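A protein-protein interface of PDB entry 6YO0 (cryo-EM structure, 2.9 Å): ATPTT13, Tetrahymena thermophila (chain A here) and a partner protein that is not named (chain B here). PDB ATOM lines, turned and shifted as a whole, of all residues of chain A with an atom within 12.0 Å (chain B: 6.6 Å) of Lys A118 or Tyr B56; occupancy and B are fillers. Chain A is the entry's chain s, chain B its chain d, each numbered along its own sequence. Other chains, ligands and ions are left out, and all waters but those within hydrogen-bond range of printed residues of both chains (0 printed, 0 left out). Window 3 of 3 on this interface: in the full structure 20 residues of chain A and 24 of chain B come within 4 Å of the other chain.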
ATOM      1  N   ASN A 115      -8.557 -27.448  -3.743  1.00  0.00           N
ATOM      2  CA  ASN A 115      -8.380 -26.940  -5.098  1.00  0.00           C
ATOM      3  C   ASN A 115      -9.599 -27.234  -5.962  1.00  0.00           C
ATOM      4  O   ASN A 115      -9.807 -26.601  -6.996  1.00  0.00           O
ATOM      5  CB  ASN A 115      -7.134 -27.551  -5.735  1.00  0.00           C
ATOM      6  CG  ASN A 115      -6.860 -27.000  -7.116  1.00  0.00           C
ATOM      7  OD1 ASN A 115      -6.235 -25.950  -7.267  1.00  0.00           O
ATOM      8  ND2 ASN A 115      -7.325 -27.709  -8.136  1.00  0.00           N
ATOM      9  N   MET A 116     -10.402 -28.209  -5.531  1.00  0.00           N
ATOM     10  CA  MET A 116     -11.641 -28.514  -6.236  1.00  0.00           C
ATOM     11  C   MET A 116     -12.521 -27.276  -6.359  1.00  0.00           C
ATOM     12  O   MET A 116     -13.189 -27.076  -7.380  1.00  0.00           O
ATOM     13  CB  MET A 116     -12.383 -29.632  -5.507  1.00  0.00           C
ATOM     14  CG  MET A 116     -13.737 -29.977  -6.097  1.00  0.00           C
ATOM     15  SD  MET A 116     -14.544 -31.350  -5.248  1.00  0.00           S
ATOM     16  CE  MET A 116     -14.593 -30.740  -3.565  1.00  0.00           C
ATOM     17  N   ALA A 117     -12.532 -26.433  -5.326  1.00  0.00           N
ATOM     18  CA  ALA A 117     -13.298 -25.193  -5.375  1.00  0.00           C
ATOM     19  C   ALA A 117     -12.859 -24.293  -6.522  1.00  0.00           C
ATOM     20  O   ALA A 117     -13.686 -23.578  -7.098  1.00  0.00           O
ATOM     21  CB  ALA A 117     -13.161 -24.446  -4.052  1.00  0.00           C
ATOM     22  N   LYS A 118     -11.574 -24.316  -6.871  1.00  0.00           N
ATOM     23  CA  LYS A 118     -11.100 -23.493  -7.978  1.00  0.00           C
ATOM     24  C   LYS A 118     -11.741 -23.910  -9.294  1.00  0.00           C
ATOM     25  O   LYS A 118     -12.170 -23.059 -10.082  1.00  0.00           O
ATOM     26  CB  LYS A 118      -9.577 -23.582  -8.066  1.00  0.00           C
ATOM     27  CG  LYS A 118      -8.973 -22.954  -9.307  1.00  0.00           C
ATOM     28  CD  LYS A 118      -7.456 -23.011  -9.254  1.00  0.00           C
ATOM     29  CE  LYS A 118      -6.832 -22.611 -10.577  1.00  0.00           C
ATOM     30  NZ  LYS A 118      -7.198 -23.547 -11.673  1.00  0.00           N
ATOM     31  N   ALA A 119     -11.815 -25.215  -9.554  1.00  0.00           N
ATOM     32  CA  ALA A 119     -12.463 -25.684 -10.773  1.00  0.00           C
ATOM     33  C   ALA A 119     -13.939 -25.308 -10.800  1.00  0.00           C
ATOM     34  O   ALA A 119     -14.457 -24.871 -11.834  1.00  0.00           O
ATOM     35  CB  ALA A 119     -12.295 -27.196 -10.903  1.00  0.00           C
ATOM     36  N   TYR A 120     -14.633 -25.468  -9.672  1.00  0.00           N
ATOM     37  CA  TYR A 120     -16.044 -25.102  -9.620  1.00  0.00           C
ATOM     38  C   TYR A 120     -16.240 -23.612  -9.862  1.00  0.00           C
ATOM     39  O   TYR A 120     -17.188 -23.206 -10.543  1.00  0.00           O
ATOM     40  CB  TYR A 120     -16.646 -25.500  -8.271  1.00  0.00           C
ATOM     41  CG  TYR A 120     -16.785 -26.992  -8.050  1.00  0.00           C
ATOM     42  CD1 TYR A 120     -16.812 -27.880  -9.118  1.00  0.00           C
ATOM     43  CD2 TYR A 120     -16.903 -27.511  -6.770  1.00  0.00           C
ATOM     44  CE1 TYR A 120     -16.940 -29.238  -8.916  1.00  0.00           C
ATOM     45  CE2 TYR A 120     -17.034 -28.869  -6.557  1.00  0.00           C
ATOM     46  CZ  TYR A 120     -17.052 -29.728  -7.633  1.00  0.00           C
ATOM     47  OH  TYR A 120     -17.182 -31.082  -7.427  1.00  0.00           O
ATOM     48  N   VAL A 121     -15.346 -22.780  -9.326  1.00  0.00           N
ATOM     49  CA  VAL A 121     -15.473 -21.339  -9.520  1.00  0.00           C
ATOM     50  C   VAL A 121     -15.373 -20.990 -10.997  1.00  0.00           C
ATOM     51  O   VAL A 121     -16.189 -20.229 -11.531  1.00  0.00           O
ATOM     52  CB  VAL A 121     -14.408 -20.596  -8.695  1.00  0.00           C
ATOM     53  CG1 VAL A 121     -14.305 -19.154  -9.136  1.00  0.00           C
ATOM     54  CG2 VAL A 121     -14.740 -20.664  -7.217  1.00  0.00           C
ATOM     55  N   HIS A 122     -14.372 -21.540 -11.682  1.00  0.00           N
ATOM     56  CA  HIS A 122     -14.217 -21.255 -13.103  1.00  0.00           C
ATOM     57  C   HIS A 122     -15.454 -21.669 -13.890  1.00  0.00           C
ATOM     58  O   HIS A 122     -15.933 -20.918 -14.749  1.00  0.00           O
ATOM     59  CB  HIS A 122     -12.970 -21.954 -13.638  1.00  0.00           C
ATOM     60  CG  HIS A 122     -11.697 -21.262 -13.270  1.00  0.00           C
ATOM     61  ND1 HIS A 122     -11.271 -21.137 -11.966  1.00  0.00           N
ATOM     62  CD2 HIS A 122     -10.763 -20.647 -14.031  1.00  0.00           C
ATOM     63  CE1 HIS A 122     -10.125 -20.481 -11.940  1.00  0.00           C
ATOM     64  NE2 HIS A 122      -9.795 -20.171 -13.180  1.00  0.00           N
ATOM     65  N   ASP A 123     -15.987 -22.860 -13.614  1.00  0.00           N
ATOM     66  CA  ASP A 123     -17.169 -23.324 -14.335  1.00  0.00           C
ATOM     67  C   ASP A 123     -18.355 -22.399 -14.100  1.00  0.00           C
ATOM     68  O   ASP A 123     -19.000 -21.940 -15.050  1.00  0.00           O
ATOM     69  CB  ASP A 123     -17.518 -24.747 -13.913  1.00  0.00           C
ATOM     70  CG  ASP A 123     -18.806 -25.231 -14.537  1.00  0.00           C
ATOM     71  OD1 ASP A 123     -18.848 -25.358 -15.778  1.00  0.00           O
ATOM     72  OD2 ASP A 123     -19.780 -25.473 -13.795  1.00  0.00           O
ATOM     73  N   ILE A 124     -18.660 -22.117 -12.832  1.00  0.00           N
ATOM     74  CA  ILE A 124     -19.818 -21.288 -12.511  1.00  0.00           C
ATOM     75  C   ILE A 124     -19.660 -19.906 -13.127  1.00  0.00           C
ATOM     76  O   ILE A 124     -20.638 -19.288 -13.565  1.00  0.00           O
ATOM     77  CB  ILE A 124     -20.026 -21.219 -10.989  1.00  0.00           C
ATOM     78  CG1 ILE A 124     -20.275 -22.614 -10.411  1.00  0.00           C
ATOM     79  CG2 ILE A 124     -21.197 -20.327 -10.659  1.00  0.00           C
ATOM     80  CD1 ILE A 124     -21.517 -23.310 -10.944  1.00  0.00           C
ATOM     81  N   CYS A 125     -18.428 -19.399 -13.174  1.00  0.00           N
ATOM     82  CA  CYS A 125     -18.213 -18.082 -13.755  1.00  0.00           C
ATOM     83  C   CYS A 125     -18.400 -18.121 -15.263  1.00  0.00           C
ATOM     84  O   CYS A 125     -18.812 -17.123 -15.861  1.00  0.00           O
ATOM     85  CB  CYS A 125     -16.814 -17.579 -13.406  1.00  0.00           C
ATOM     86  SG  CYS A 125     -16.441 -15.928 -14.037  1.00  0.00           S
ATOM     87  N   GLY A 126     -18.100 -19.258 -15.890  1.00  0.00           N
ATOM     88  CA  GLY A 126     -18.265 -19.365 -17.328  1.00  0.00           C
ATOM     89  C   GLY A 126     -19.676 -19.044 -17.777  1.00  0.00           C
ATOM     90  O   GLY A 126     -19.873 -18.472 -18.853  1.00  0.00           O
ATOM     91  N   TYR A 127     -20.674 -19.402 -16.967  1.00  0.00           N
ATOM     92  CA  TYR A 127     -22.076 -19.255 -17.331  1.00  0.00           C
ATOM     93  C   TYR A 127     -22.678 -17.950 -16.826  1.00  0.00           C
ATOM     94  O   TYR A 127     -23.907 -17.824 -16.767  1.00  0.00           O
ATOM     95  CB  TYR A 127     -22.881 -20.442 -16.798  1.00  0.00           C
ATOM     96  CG  TYR A 127     -22.672 -21.742 -17.551  1.00  0.00           C
ATOM     97  CD1 TYR A 127     -23.030 -22.956 -16.982  1.00  0.00           C
ATOM     98  CD2 TYR A 127     -22.117 -21.758 -18.828  1.00  0.00           C
ATOM     99  CE1 TYR A 127     -22.842 -24.148 -17.661  1.00  0.00           C
ATOM    100  CE2 TYR A 127     -21.929 -22.943 -19.512  1.00  0.00           C
ATOM    101  CZ  TYR A 127     -22.292 -24.133 -18.926  1.00  0.00           C
ATOM    102  OH  TYR A 127     -22.102 -25.312 -19.612  1.00  0.00           O
ATOM    103  N   LEU B  44     -18.185 -27.376   1.871  1.00  0.00           N
ATOM    104  CA  LEU B  44     -17.027 -27.123   1.023  1.00  0.00           C
ATOM    105  C   LEU B  44     -16.054 -26.156   1.686  1.00  0.00           C
ATOM    106  O   LEU B  44     -14.834 -26.314   1.563  1.00  0.00           O
ATOM    107  CB  LEU B  44     -17.497 -26.582  -0.325  1.00  0.00           C
ATOM    108  CG  LEU B  44     -16.473 -26.474  -1.456  1.00  0.00           C
ATOM    109  CD1 LEU B  44     -15.572 -25.271  -1.252  1.00  0.00           C
ATOM    110  CD2 LEU B  44     -15.646 -27.744  -1.560  1.00  0.00           C
ATOM    111  N   GLY B  51      -4.918 -20.909   3.230  1.00  0.00           N
ATOM    112  CA  GLY B  51      -5.401 -19.577   2.916  1.00  0.00           C
ATOM    113  C   GLY B  51      -5.895 -19.471   1.487  1.00  0.00           C
ATOM    114  O   GLY B  51      -6.935 -18.864   1.221  1.00  0.00           O
ATOM    115  N   GLU B  52      -5.154 -20.061   0.546  1.00  0.00           N
ATOM    116  CA  GLU B  52      -5.614 -20.093  -0.836  1.00  0.00           C
ATOM    117  C   GLU B  52      -6.937 -20.837  -0.959  1.00  0.00           C
ATOM    118  O   GLU B  52      -7.856 -20.373  -1.644  1.00  0.00           O
ATOM    119  CB  GLU B  52      -4.551 -20.747  -1.719  1.00  0.00           C
ATOM    120  CG  GLU B  52      -4.978 -20.980  -3.159  1.00  0.00           C
ATOM    121  CD  GLU B  52      -3.968 -21.795  -3.939  1.00  0.00           C
ATOM    122  OE1 GLU B  52      -2.949 -22.205  -3.345  1.00  0.00           O
ATOM    123  OE2 GLU B  52      -4.195 -22.029  -5.145  1.00  0.00           O
ATOM    124  N   SER B  53      -7.063 -21.982  -0.285  1.00  0.00           N
ATOM    125  CA  SER B  53      -8.325 -22.713  -0.317  1.00  0.00           C
ATOM    126  C   SER B  53      -9.460 -21.876   0.255  1.00  0.00           C
ATOM    127  O   SER B  53     -10.576 -21.883  -0.275  1.00  0.00           O
ATOM    128  CB  SER B  53      -8.185 -24.023   0.455  1.00  0.00           C
ATOM    129  OG  SER B  53      -7.866 -23.777   1.814  1.00  0.00           O
ATOM    130  N   ARG B  54      -9.191 -21.142   1.333  1.00  0.00           N
ATOM    131  CA  ARG B  54     -10.217 -20.289   1.922  1.00  0.00           C
ATOM    132  C   ARG B  54     -10.610 -19.164   0.973  1.00  0.00           C
ATOM    133  O   ARG B  54     -11.792 -18.820   0.864  1.00  0.00           O
ATOM    134  CB  ARG B  54      -9.724 -19.727   3.252  1.00  0.00           C
ATOM    135  CG  ARG B  54      -9.408 -20.795   4.282  1.00  0.00           C
ATOM    136  CD  ARG B  54      -8.814 -20.192   5.533  1.00  0.00           C
ATOM    137  NE  ARG B  54      -9.754 -19.299   6.201  1.00  0.00           N
ATOM    138  CZ  ARG B  54      -9.457 -18.568   7.271  1.00  0.00           C
ATOM    139  NH1 ARG B  54     -10.380 -17.785   7.813  1.00  0.00           N
ATOM    140  NH2 ARG B  54      -8.239 -18.612   7.794  1.00  0.00           N
ATOM    141  N   SER B  55      -9.632 -18.585   0.274  1.00  0.00           N
ATOM    142  CA  SER B  55      -9.934 -17.521  -0.675  1.00  0.00           C
ATOM    143  C   SER B  55     -10.791 -18.030  -1.824  1.00  0.00           C
ATOM    144  O   SER B  55     -11.722 -17.348  -2.262  1.00  0.00           O
ATOM    145  CB  SER B  55      -8.640 -16.911  -1.212  1.00  0.00           C
ATOM    146  OG  SER B  55      -7.880 -17.877  -1.911  1.00  0.00           O
ATOM    147  N   TYR B  56     -10.502 -19.232  -2.322  1.00  0.00           N
ATOM    148  CA  TYR B  56     -11.317 -19.781  -3.398  1.00  0.00           C
ATOM    149  C   TYR B  56     -12.748 -20.018  -2.937  1.00  0.00           C
ATOM    150  O   TYR B  56     -13.695 -19.829  -3.708  1.00  0.00           O
ATOM    151  CB  TYR B  56     -10.696 -21.073  -3.925  1.00  0.00           C
ATOM    152  CG  TYR B  56      -9.612 -20.829  -4.947  1.00  0.00           C
ATOM    153  CD1 TYR B  56      -9.927 -20.620  -6.279  1.00  0.00           C
ATOM    154  CD2 TYR B  56      -8.276 -20.801  -4.579  1.00  0.00           C
ATOM    155  CE1 TYR B  56      -8.944 -20.389  -7.217  1.00  0.00           C
ATOM    156  CE2 TYR B  56      -7.286 -20.575  -5.509  1.00  0.00           C
ATOM    157  CZ  TYR B  56      -7.623 -20.369  -6.826  1.00  0.00           C
ATOM    158  OH  TYR B  56      -6.639 -20.142  -7.760  1.00  0.00           O
ATOM    159  N   CYS B  57     -12.929 -20.426  -1.682  1.00  0.00           N
ATOM    160  CA  CYS B  57     -14.281 -20.589  -1.160  1.00  0.00           C
ATOM    161  C   CYS B  57     -15.003 -19.250  -1.072  1.00  0.00           C
ATOM    162  O   CYS B  57     -16.211 -19.173  -1.322  1.00  0.00           O
ATOM    163  CB  CYS B  57     -14.234 -21.261   0.210  1.00  0.00           C
ATOM    164  SG  CYS B  57     -13.751 -22.995   0.160  1.00  0.00           S
ATOM    165  N   THR B  58     -14.280 -18.183  -0.721  1.00  0.00           N
ATOM    166  CA  THR B  58     -14.889 -16.855  -0.711  1.00  0.00           C
ATOM    167  C   THR B  58     -15.381 -16.472  -2.098  1.00  0.00           C
ATOM    168  O   THR B  58     -16.484 -15.935  -2.250  1.00  0.00           O
ATOM    169  CB  THR B  58     -13.890 -15.814  -0.206  1.00  0.00           C
ATOM    170  OG1 THR B  58     -12.848 -15.642  -1.171  1.00  0.00           O
ATOM    171  CG2 THR B  58     -13.277 -16.245   1.121  1.00  0.00           C
ATOM    172  N   GLN B  59     -14.574 -16.743  -3.124  1.00  0.00           N
ATOM    173  CA  GLN B  59     -14.989 -16.442  -4.487  1.00  0.00           C
ATOM    174  C   GLN B  59     -16.230 -17.239  -4.860  1.00  0.00           C
ATOM    175  O   GLN B  59     -17.165 -16.707  -5.470  1.00  0.00           O
ATOM    176  CB  GLN B  59     -13.847 -16.754  -5.452  1.00  0.00           C
ATOM    177  CG  GLN B  59     -12.533 -16.065  -5.119  1.00  0.00           C
ATOM    178  CD  GLN B  59     -11.407 -16.398  -6.084  1.00  0.00           C
ATOM    179  OE1 GLN B  59     -10.263 -16.004  -5.864  1.00  0.00           O
ATOM    180  NE2 GLN B  59     -11.717 -17.129  -7.148  1.00  0.00           N
ATOM    181  N   LEU B  60     -16.254 -18.517  -4.490  1.00  0.00           N
ATOM    182  CA  LEU B  60     -17.405 -19.363  -4.780  1.00  0.00           C
ATOM    183  C   LEU B  60     -18.665 -18.840  -4.103  1.00  0.00           C
ATOM    184  O   LEU B  60     -19.733 -18.779  -4.722  1.00  0.00           O
ATOM    185  CB  LEU B  60     -17.105 -20.795  -4.337  1.00  0.00           C
ATOM    186  CG  LEU B  60     -18.093 -21.905  -4.692  1.00  0.00           C
ATOM    187  CD1 LEU B  60     -19.358 -21.831  -3.857  1.00  0.00           C
ATOM    188  CD2 LEU B  60     -18.420 -21.855  -6.170  1.00  0.00           C
ATOM    189  N   SER B  61     -18.559 -18.453  -2.831  1.00  0.00           N
ATOM    190  CA  SER B  61     -19.725 -17.959  -2.103  1.00  0.00           C
ATOM    191  C   SER B  61     -20.260 -16.666  -2.705  1.00  0.00           C
ATOM    192  O   SER B  61     -21.477 -16.454  -2.748  1.00  0.00           O
ATOM    193  CB  SER B  61     -19.367 -17.752  -0.634  1.00  0.00           C
ATOM    194  OG  SER B  61     -20.477 -17.264   0.094  1.00  0.00           O
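The backbone carbonyl oxygen (O) of Leu B44 lies close to the side-chain sulfur (SG) of Cys B57, at 3.8 Å. The backbone carbonyl oxygen of Lys A118 lies within hydrogen-bond range of a ring nitrogen (ND1) of His A122, 2.8 Å away. The side-chain hydroxyl of Tyr A120 is in hydrogen-bond range of the side-chain sulfur of Met A116 (3.4 Å).
CE of Met A116 touches CD2 of Leu B44, at 3.8 Å. CB of Ala A117 touches CD1 of Leu B44, 3.8 Å away. CE1 of Tyr B56 touches CG of Lys A118 (3.3 Å). CG2 of Val A121 touches O of Tyr B56, at 3.8 Å. Gln B59 touches Val A121. Val A121 touches Leu B60 (CG2 to CB, 3.7 Å).
Of the printed residues of chain B, Met A116 touches Leu B44 (3.8 Å). Of the printed residues of chain B, Ala A117 touches Leu B44 (3.8 Å). Lys A118 touches just one residue of chain B: Tyr B56 (3.3 Å). Printed residues of chain B within 4 Å of Val A121: Tyr B56 (3.8 Å), Gln B59 (3.8 Å) and Leu B60 (3.7 Å). Gly A126 touches none of the printed residues of chain B. Of the printed residues of chain A, Leu B44 touches Met A116 (3.8 Å) and Ala A117 (3.8 Å). Gly B51 touches none of the printed residues of chain A. No residue of chain A comes within 4 Å of Glu B52. No residue of chain A comes within 4 Å of Ser B55. Of the printed residues of chain A, Tyr B56 touches Lys A118 and Val A121. No residue of chain A comes within 4 Å of Cys B57. No residue of chain A comes within 4 Å of Thr B58. Of chain A, only Val A121 comes within 4 Å of Leu B60. The nearest printed residue of chain B that does not touch Ala A117 is Tyr B56 (4.2 Å).
Printed residues of chain A that touch a printed residue of chain B: Met A116, Ala A117, Lys A118 and Val A121. Hydrophobic or aromatic side chains of chain A that line the printed part of chain B: Met A116, Ala A117 and Val A121. Of the 12 printed residues of chain B, 4 touch a printed residue of chain A. Hydrophobic or aromatic side chains of chain B that line the printed part of chain A: Leu B44, Tyr B56 and Leu B60. Among the printed residues, no Asp or Glu carboxylate lies within 4 Å of a Lys or Arg side-chain nitrogen of the other chain.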
